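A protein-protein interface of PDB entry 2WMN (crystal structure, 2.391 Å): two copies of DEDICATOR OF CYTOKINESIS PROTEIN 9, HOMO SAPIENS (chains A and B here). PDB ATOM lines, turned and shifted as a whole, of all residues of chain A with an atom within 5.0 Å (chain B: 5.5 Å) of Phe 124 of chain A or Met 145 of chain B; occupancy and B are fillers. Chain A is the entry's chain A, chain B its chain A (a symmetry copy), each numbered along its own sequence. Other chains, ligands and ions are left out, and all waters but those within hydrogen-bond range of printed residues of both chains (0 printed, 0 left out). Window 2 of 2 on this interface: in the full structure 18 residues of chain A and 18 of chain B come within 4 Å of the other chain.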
ATOM      1  N   ARG A 122     -13.523  -3.625  -9.831  1.00  0.00           N
ATOM      2  CA  ARG A 122     -14.185  -4.716  -9.123  1.00  0.00           C
ATOM      3  C   ARG A 122     -13.228  -5.880  -8.843  1.00  0.00           C
ATOM      4  O   ARG A 122     -13.582  -7.046  -8.930  1.00  0.00           O
ATOM      5  CB  ARG A 122     -15.471  -5.169  -9.850  1.00  0.00           C
ATOM      6  CG  ARG A 122     -16.327  -4.007 -10.401  1.00  0.00           C
ATOM      7  CD  ARG A 122     -17.759  -4.436 -10.677  1.00  0.00           C
ATOM      8  NE  ARG A 122     -18.455  -3.604 -11.660  1.00  0.00           N
ATOM      9  CZ  ARG A 122     -18.719  -2.307 -11.512  1.00  0.00           C
ATOM     10  NH1 ARG A 122     -19.370  -1.658 -12.472  1.00  0.00           N
ATOM     11  NH2 ARG A 122     -18.314  -1.644 -10.425  1.00  0.00           N
ATOM     12  N   ASP A 123     -12.004  -5.556  -8.471  1.00  0.00           N
ATOM     13  CA  ASP A 123     -11.044  -6.609  -8.177  1.00  0.00           C
ATOM     14  C   ASP A 123     -11.108  -7.012  -6.711  1.00  0.00           C
ATOM     15  O   ASP A 123     -10.314  -6.558  -5.897  1.00  0.00           O
ATOM     16  CB  ASP A 123      -9.638  -6.181  -8.558  1.00  0.00           C
ATOM     17  CG  ASP A 123      -8.711  -7.357  -8.714  1.00  0.00           C
ATOM     18  OD1 ASP A 123      -8.933  -8.387  -8.027  1.00  0.00           O
ATOM     19  OD2 ASP A 123      -7.757  -7.257  -9.526  1.00  0.00           O
ATOM     20  N   PHE A 124     -12.067  -7.859  -6.374  1.00  0.00           N
ATOM     21  CA  PHE A 124     -12.293  -8.192  -4.977  1.00  0.00           C
ATOM     22  C   PHE A 124     -11.192  -9.041  -4.353  1.00  0.00           C
ATOM     23  O   PHE A 124     -10.961  -8.949  -3.143  1.00  0.00           O
ATOM     24  CB  PHE A 124     -13.663  -8.867  -4.799  1.00  0.00           C
ATOM     25  CG  PHE A 124     -14.793  -8.107  -5.437  1.00  0.00           C
ATOM     26  CD1 PHE A 124     -15.188  -6.872  -4.930  1.00  0.00           C
ATOM     27  CD2 PHE A 124     -15.454  -8.617  -6.556  1.00  0.00           C
ATOM     28  CE1 PHE A 124     -16.226  -6.162  -5.532  1.00  0.00           C
ATOM     29  CE2 PHE A 124     -16.461  -7.903  -7.169  1.00  0.00           C
ATOM     30  CZ  PHE A 124     -16.861  -6.687  -6.650  1.00  0.00           C
ATOM     31  N   GLU A 125     -10.542  -9.879  -5.159  1.00  0.00           N
ATOM     32  CA  GLU A 125      -9.441 -10.728  -4.693  1.00  0.00           C
ATOM     33  C   GLU A 125      -8.268  -9.866  -4.223  1.00  0.00           C
ATOM     34  O   GLU A 125      -7.746 -10.078  -3.135  1.00  0.00           O
ATOM     35  CB  GLU A 125      -8.973 -11.670  -5.812  1.00  0.00           C
ATOM     36  CG  GLU A 125      -8.035 -12.791  -5.349  1.00  0.00           C
ATOM     37  CD  GLU A 125      -6.539 -12.412  -5.369  1.00  0.00           C
ATOM     38  OE1 GLU A 125      -5.961 -12.242  -6.477  1.00  0.00           O
ATOM     39  OE2 GLU A 125      -5.931 -12.307  -4.273  1.00  0.00           O
ATOM     40  N   ARG A 126      -7.897  -8.877  -5.033  1.00  0.00           N
ATOM     41  CA  ARG A 126      -6.868  -7.897  -4.688  1.00  0.00           C
ATOM     42  C   ARG A 126      -7.220  -7.130  -3.433  1.00  0.00           C
ATOM     43  O   ARG A 126      -6.351  -6.871  -2.593  1.00  0.00           O
ATOM     44  CB  ARG A 126      -6.675  -6.874  -5.811  1.00  0.00           C
ATOM     45  CG  ARG A 126      -6.079  -7.394  -7.116  1.00  0.00           C
ATOM     46  CD  ARG A 126      -4.868  -8.279  -6.928  1.00  0.00           C
ATOM     47  NE  ARG A 126      -3.919  -8.153  -8.038  1.00  0.00           N
ATOM     48  CZ  ARG A 126      -4.124  -8.593  -9.288  1.00  0.00           C
ATOM     49  NH1 ARG A 126      -5.281  -9.172  -9.636  1.00  0.00           N
ATOM     50  NH2 ARG A 126      -3.171  -8.433 -10.208  1.00  0.00           N
ATOM     51  N   LEU A 127      -8.492  -6.740  -3.316  1.00  0.00           N
ATOM     52  CA  LEU A 127      -8.921  -5.943  -2.161  1.00  0.00           C
ATOM     53  C   LEU A 127      -8.800  -6.797  -0.923  1.00  0.00           C
ATOM     54  O   LEU A 127      -8.369  -6.323   0.118  1.00  0.00           O
ATOM     55  CB  LEU A 127     -10.346  -5.403  -2.323  1.00  0.00           C
ATOM     56  CG  LEU A 127     -10.484  -4.297  -3.363  1.00  0.00           C
ATOM     57  CD1 LEU A 127     -11.892  -4.258  -3.870  1.00  0.00           C
ATOM     58  CD2 LEU A 127     -10.047  -2.929  -2.854  1.00  0.00           C
ATOM     59  N   ALA A 128      -9.164  -8.068  -1.050  1.00  0.00           N
ATOM     60  CA  ALA A 128      -9.079  -9.004   0.073  1.00  0.00           C
ATOM     61  C   ALA A 128      -7.642  -9.076   0.574  1.00  0.00           C
ATOM     62  O   ALA A 128      -7.381  -9.020   1.774  1.00  0.00           O
ATOM     63  CB  ALA A 128      -9.569 -10.404  -0.352  1.00  0.00           C
ATOM     64  N   GLU B 105     -20.005  -5.765   0.077  1.00  0.00           N
ATOM     65  CA  GLU B 105     -19.492  -4.729  -0.801  1.00  0.00           C
ATOM     66  C   GLU B 105     -19.605  -3.304  -0.280  1.00  0.00           C
ATOM     67  O   GLU B 105     -18.990  -2.399  -0.847  1.00  0.00           O
ATOM     68  CB  GLU B 105     -20.250  -4.806  -2.131  1.00  0.00           C
ATOM     69  CG  GLU B 105     -19.893  -5.995  -2.967  1.00  0.00           C
ATOM     70  CD  GLU B 105     -20.731  -7.217  -2.666  1.00  0.00           C
ATOM     71  OE1 GLU B 105     -21.410  -7.266  -1.618  1.00  0.00           O
ATOM     72  OE2 GLU B 105     -20.689  -8.134  -3.504  1.00  0.00           O
ATOM     73  N   TYR B 138     -14.398  -9.035   1.841  1.00  0.00           N
ATOM     74  CA  TYR B 138     -14.035  -9.203   0.422  1.00  0.00           C
ATOM     75  C   TYR B 138     -13.753 -10.659   0.108  1.00  0.00           C
ATOM     76  O   TYR B 138     -13.820 -11.102  -1.040  1.00  0.00           O
ATOM     77  CB  TYR B 138     -12.888  -8.265  -0.014  1.00  0.00           C
ATOM     78  CG  TYR B 138     -13.393  -6.852  -0.205  1.00  0.00           C
ATOM     79  CD1 TYR B 138     -14.068  -6.488  -1.363  1.00  0.00           C
ATOM     80  CD2 TYR B 138     -13.249  -5.909   0.791  1.00  0.00           C
ATOM     81  CE1 TYR B 138     -14.573  -5.233  -1.527  1.00  0.00           C
ATOM     82  CE2 TYR B 138     -13.730  -4.637   0.628  1.00  0.00           C
ATOM     83  CZ  TYR B 138     -14.402  -4.303  -0.535  1.00  0.00           C
ATOM     84  OH  TYR B 138     -14.905  -3.023  -0.711  1.00  0.00           O
ATOM     85  N   LYS B 140     -15.689 -13.148   1.614  1.00  0.00           N
ATOM     86  CA  LYS B 140     -17.072 -13.579   1.394  1.00  0.00           C
ATOM     87  C   LYS B 140     -17.541 -13.272  -0.027  1.00  0.00           C
ATOM     88  O   LYS B 140     -18.116 -14.128  -0.710  1.00  0.00           O
ATOM     89  CB  LYS B 140     -18.002 -12.914   2.400  1.00  0.00           C
ATOM     90  CG  LYS B 140     -18.136 -13.662   3.709  1.00  0.00           C
ATOM     91  CD  LYS B 140     -18.294 -15.146   3.432  1.00  0.00           C
ATOM     92  CE  LYS B 140     -19.139 -15.840   4.484  1.00  0.00           C
ATOM     93  NZ  LYS B 140     -20.013 -16.856   3.826  1.00  0.00           N
ATOM     94  N   VAL B 141     -17.269 -12.050  -0.474  1.00  0.00           N
ATOM     95  CA  VAL B 141     -17.680 -11.603  -1.795  1.00  0.00           C
ATOM     96  C   VAL B 141     -17.271 -12.551  -2.925  1.00  0.00           C
ATOM     97  O   VAL B 141     -18.111 -12.934  -3.743  1.00  0.00           O
ATOM     98  CB  VAL B 141     -17.151 -10.182  -2.099  1.00  0.00           C
ATOM     99  CG1 VAL B 141     -17.277  -9.865  -3.562  1.00  0.00           C
ATOM    100  CG2 VAL B 141     -17.877  -9.167  -1.277  1.00  0.00           C
ATOM    101  N   THR B 142     -15.993 -12.930  -3.003  1.00  0.00           N
ATOM    102  CA  THR B 142     -15.614 -13.898  -4.038  1.00  0.00           C
ATOM    103  C   THR B 142     -16.294 -15.249  -3.808  1.00  0.00           C
ATOM    104  O   THR B 142     -16.671 -15.916  -4.759  1.00  0.00           O
ATOM    105  CB  THR B 142     -14.081 -14.106  -4.171  1.00  0.00           C
ATOM    106  OG1 THR B 142     -13.522 -14.413  -2.883  1.00  0.00           O
ATOM    107  CG2 THR B 142     -13.410 -12.863  -4.757  1.00  0.00           C
ATOM    108  N   GLU B 143     -16.418 -15.665  -2.553  1.00  0.00           N
ATOM    109  CA  GLU B 143     -17.100 -16.914  -2.268  1.00  0.00           C
ATOM    110  C   GLU B 143     -18.467 -16.918  -2.940  1.00  0.00           C
ATOM    111  O   GLU B 143     -18.693 -17.649  -3.900  1.00  0.00           O
ATOM    112  CB  GLU B 143     -17.309 -17.097  -0.767  1.00  0.00           C
ATOM    113  CG  GLU B 143     -16.078 -17.465  -0.002  1.00  0.00           C
ATOM    114  CD  GLU B 143     -16.359 -17.591   1.484  1.00  0.00           C
ATOM    115  OE1 GLU B 143     -17.458 -18.106   1.846  1.00  0.00           O
ATOM    116  OE2 GLU B 143     -15.482 -17.165   2.282  1.00  0.00           O
ATOM    117  N   VAL B 144     -19.359 -16.071  -2.427  1.00  0.00           N
ATOM    118  CA  VAL B 144     -20.759 -16.034  -2.847  1.00  0.00           C
ATOM    119  C   VAL B 144     -20.948 -15.644  -4.304  1.00  0.00           C
ATOM    120  O   VAL B 144     -21.965 -15.988  -4.886  1.00  0.00           O
ATOM    121  CB  VAL B 144     -21.574 -15.084  -1.967  1.00  0.00           C
ATOM    122  CG1 VAL B 144     -21.367 -15.417  -0.507  1.00  0.00           C
ATOM    123  CG2 VAL B 144     -21.160 -13.650  -2.232  1.00  0.00           C
ATOM    124  N   MET B 145     -19.984 -14.936  -4.900  1.00  0.00           N
ATOM    125  CA  MET B 145     -20.061 -14.624  -6.330  1.00  0.00           C
ATOM    126  C   MET B 145     -19.941 -15.940  -7.089  1.00  0.00           C
ATOM    127  O   MET B 145     -20.401 -16.073  -8.226  1.00  0.00           O
ATOM    128  CB  MET B 145     -18.952 -13.658  -6.790  1.00  0.00           C
ATOM    129  CG  MET B 145     -19.052 -12.224  -6.275  1.00  0.00           C
ATOM    130  SD  MET B 145     -17.958 -11.061  -7.100  1.00  0.00           S
ATOM    131  CE  MET B 145     -18.364 -11.324  -8.801  1.00  0.00           C
ATOM    132  N   HIS B 146     -19.315 -16.919  -6.445  1.00  0.00           N
ATOM    133  CA  HIS B 146     -19.085 -18.208  -7.070  1.00  0.00           C
ATOM    134  C   HIS B 146     -20.064 -19.288  -6.592  1.00  0.00           C
ATOM    135  O   HIS B 146     -20.539 -20.092  -7.385  1.00  0.00           O
ATOM    136  CB  HIS B 146     -17.642 -18.687  -6.845  1.00  0.00           C
ATOM    137  CG  HIS B 146     -17.509 -20.179  -6.895  1.00  0.00           C
ATOM    138  ND1 HIS B 146     -17.389 -20.873  -8.082  1.00  0.00           N
ATOM    139  CD2 HIS B 146     -17.549 -21.111  -5.912  1.00  0.00           C
ATOM    140  CE1 HIS B 146     -17.330 -22.171  -7.823  1.00  0.00           C
ATOM    141  NE2 HIS B 146     -17.425 -22.339  -6.515  1.00  0.00           N
ATOM    142  N   SER B 147     -20.348 -19.310  -5.297  1.00  0.00           N
ATOM    143  CA  SER B 147     -21.213 -20.331  -4.728  1.00  0.00           C
ATOM    144  C   SER B 147     -22.706 -19.985  -4.801  1.00  0.00           C
ATOM    145  O   SER B 147     -23.548 -20.809  -4.457  1.00  0.00           O
ATOM    146  CB  SER B 147     -20.852 -20.573  -3.273  1.00  0.00           C
ATOM    147  OG  SER B 147     -21.381 -19.539  -2.474  1.00  0.00           O
ATOM    148  N   GLY B 148     -23.021 -18.763  -5.228  1.00  0.00           N
ATOM    149  CA  GLY B 148     -24.388 -18.278  -5.283  1.00  0.00           C
ATOM    150  C   GLY B 148     -25.211 -18.548  -4.033  1.00  0.00           C
ATOM    151  O   GLY B 148     -26.400 -18.840  -4.108  1.00  0.00           O
ATOM    152  N   ARG B 150     -25.456 -16.309  -1.498  1.00  0.00           N
ATOM    153  CA  ARG B 150     -26.054 -15.103  -0.951  1.00  0.00           C
ATOM    154  C   ARG B 150     -27.429 -14.858  -1.579  1.00  0.00           C
ATOM    155  O   ARG B 150     -27.534 -14.672  -2.795  1.00  0.00           O
ATOM    156  CB  ARG B 150     -25.163 -13.885  -1.138  1.00  0.00           C
ATOM    157  CG  ARG B 150     -25.767 -12.687  -0.457  1.00  0.00           C
ATOM    158  CD  ARG B 150     -24.811 -11.529  -0.449  1.00  0.00           C
ATOM    159  NE  ARG B 150     -24.195 -11.293  -1.752  1.00  0.00           N
ATOM    160  CZ  ARG B 150     -23.301 -10.332  -1.953  1.00  0.00           C
ATOM    161  NH1 ARG B 150     -22.942  -9.550  -0.940  1.00  0.00           N
ATOM    162  NH2 ARG B 150     -22.763 -10.144  -3.142  1.00  0.00           N
ATOM    163  N   THR B 244     -21.926  -6.567 -11.707  1.00  0.00           N
ATOM    164  CA  THR B 244     -22.113  -7.696 -10.818  1.00  0.00           C
ATOM    165  C   THR B 244     -23.583  -7.938 -10.454  1.00  0.00           C
ATOM    166  O   THR B 244     -24.431  -7.035 -10.530  1.00  0.00           O
ATOM    167  CB  THR B 244     -21.317  -7.486  -9.540  1.00  0.00           C
ATOM    168  OG1 THR B 244     -21.938  -6.443  -8.773  1.00  0.00           O
ATOM    169  CG2 THR B 244     -19.845  -7.100  -9.882  1.00  0.00           C
ATOM    170  N   GLU B 247     -24.594  -5.607  -7.775  1.00  0.00           N
ATOM    171  CA  GLU B 247     -24.981  -4.272  -8.190  1.00  0.00           C
ATOM    172  C   GLU B 247     -26.410  -4.285  -8.756  1.00  0.00           C
ATOM    173  O   GLU B 247     -27.076  -3.260  -8.822  1.00  0.00           O
ATOM    174  CB  GLU B 247     -23.977  -3.694  -9.184  1.00  0.00           C
ATOM    175  CG  GLU B 247     -22.670  -3.319  -8.518  1.00  0.00           C
ATOM    176  CD  GLU B 247     -21.499  -3.168  -9.496  1.00  0.00           C
ATOM    177  OE1 GLU B 247     -21.725  -2.914 -10.697  1.00  0.00           O
ATOM    178  OE2 GLU B 247     -20.341  -3.297  -9.051  1.00  0.00           O
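N of Glu 247 of chain B lies within hydrogen-bond range of OG1 of Thr 244 of chain B (3.0 Å).
Printed residues of chain B within 4 Å of Phe 124 of chain A: Tyr 138 (3.7 Å), Val 141 (3.6 Å) and Met 145 (3.5 Å). Of chain A, only Phe 124 (3.5 Å) comes within 4 Å of Met 145 of chain B. Printed residues of chain A within 4 Å of Thr 244 of chain B: Arg 122 (3.5 Å). Of the printed residues of chain B, Ala 128 of chain A touches Tyr 138. The nearest printed residue of chain B that does not touch Phe 124 of chain A is Thr 142 of chain B (4.004 Å).
No position is printed for both chains.
Among the printed residues, merely in contact across the chains: Arg 122 of chain A with Thr 244 of chain B, Phe 124 of chain A with Tyr 138 of chain B, Phe 124 of chain A with Val 141 of chain B, Phe 124 of chain A with Met 145 of chain B, Leu 127 of chain A with Tyr 138 of chain B and Ala 128 of chain A with Tyr 138 of chain B.
Hydrophobic or aromatic side chains of chain A that line the printed part of chain B: Phe 124, Leu 127 and Ala 128. Along chain A the printed residues that touch a printed residue of chain B span positions 122 to 128. Of the 14 printed residues of chain B, 5 touch a printed residue of chain A. Printed residues of chain B that touch a printed residue of chain A: Tyr 138, Val 141, Met 145, Thr 244 and Glu 247. Hydrophobic or aromatic side chains of chain B that line the printed part of chain A: Tyr 138, Val 141 and Met 145. Along chain B the printed residues that touch a printed residue of chain A span positions 138 to 247.
The guanidinium group of Arg 122 of chain A is in salt-bridge range of the side-chain carboxylate of Glu 247 of chain B (3.0 Å).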
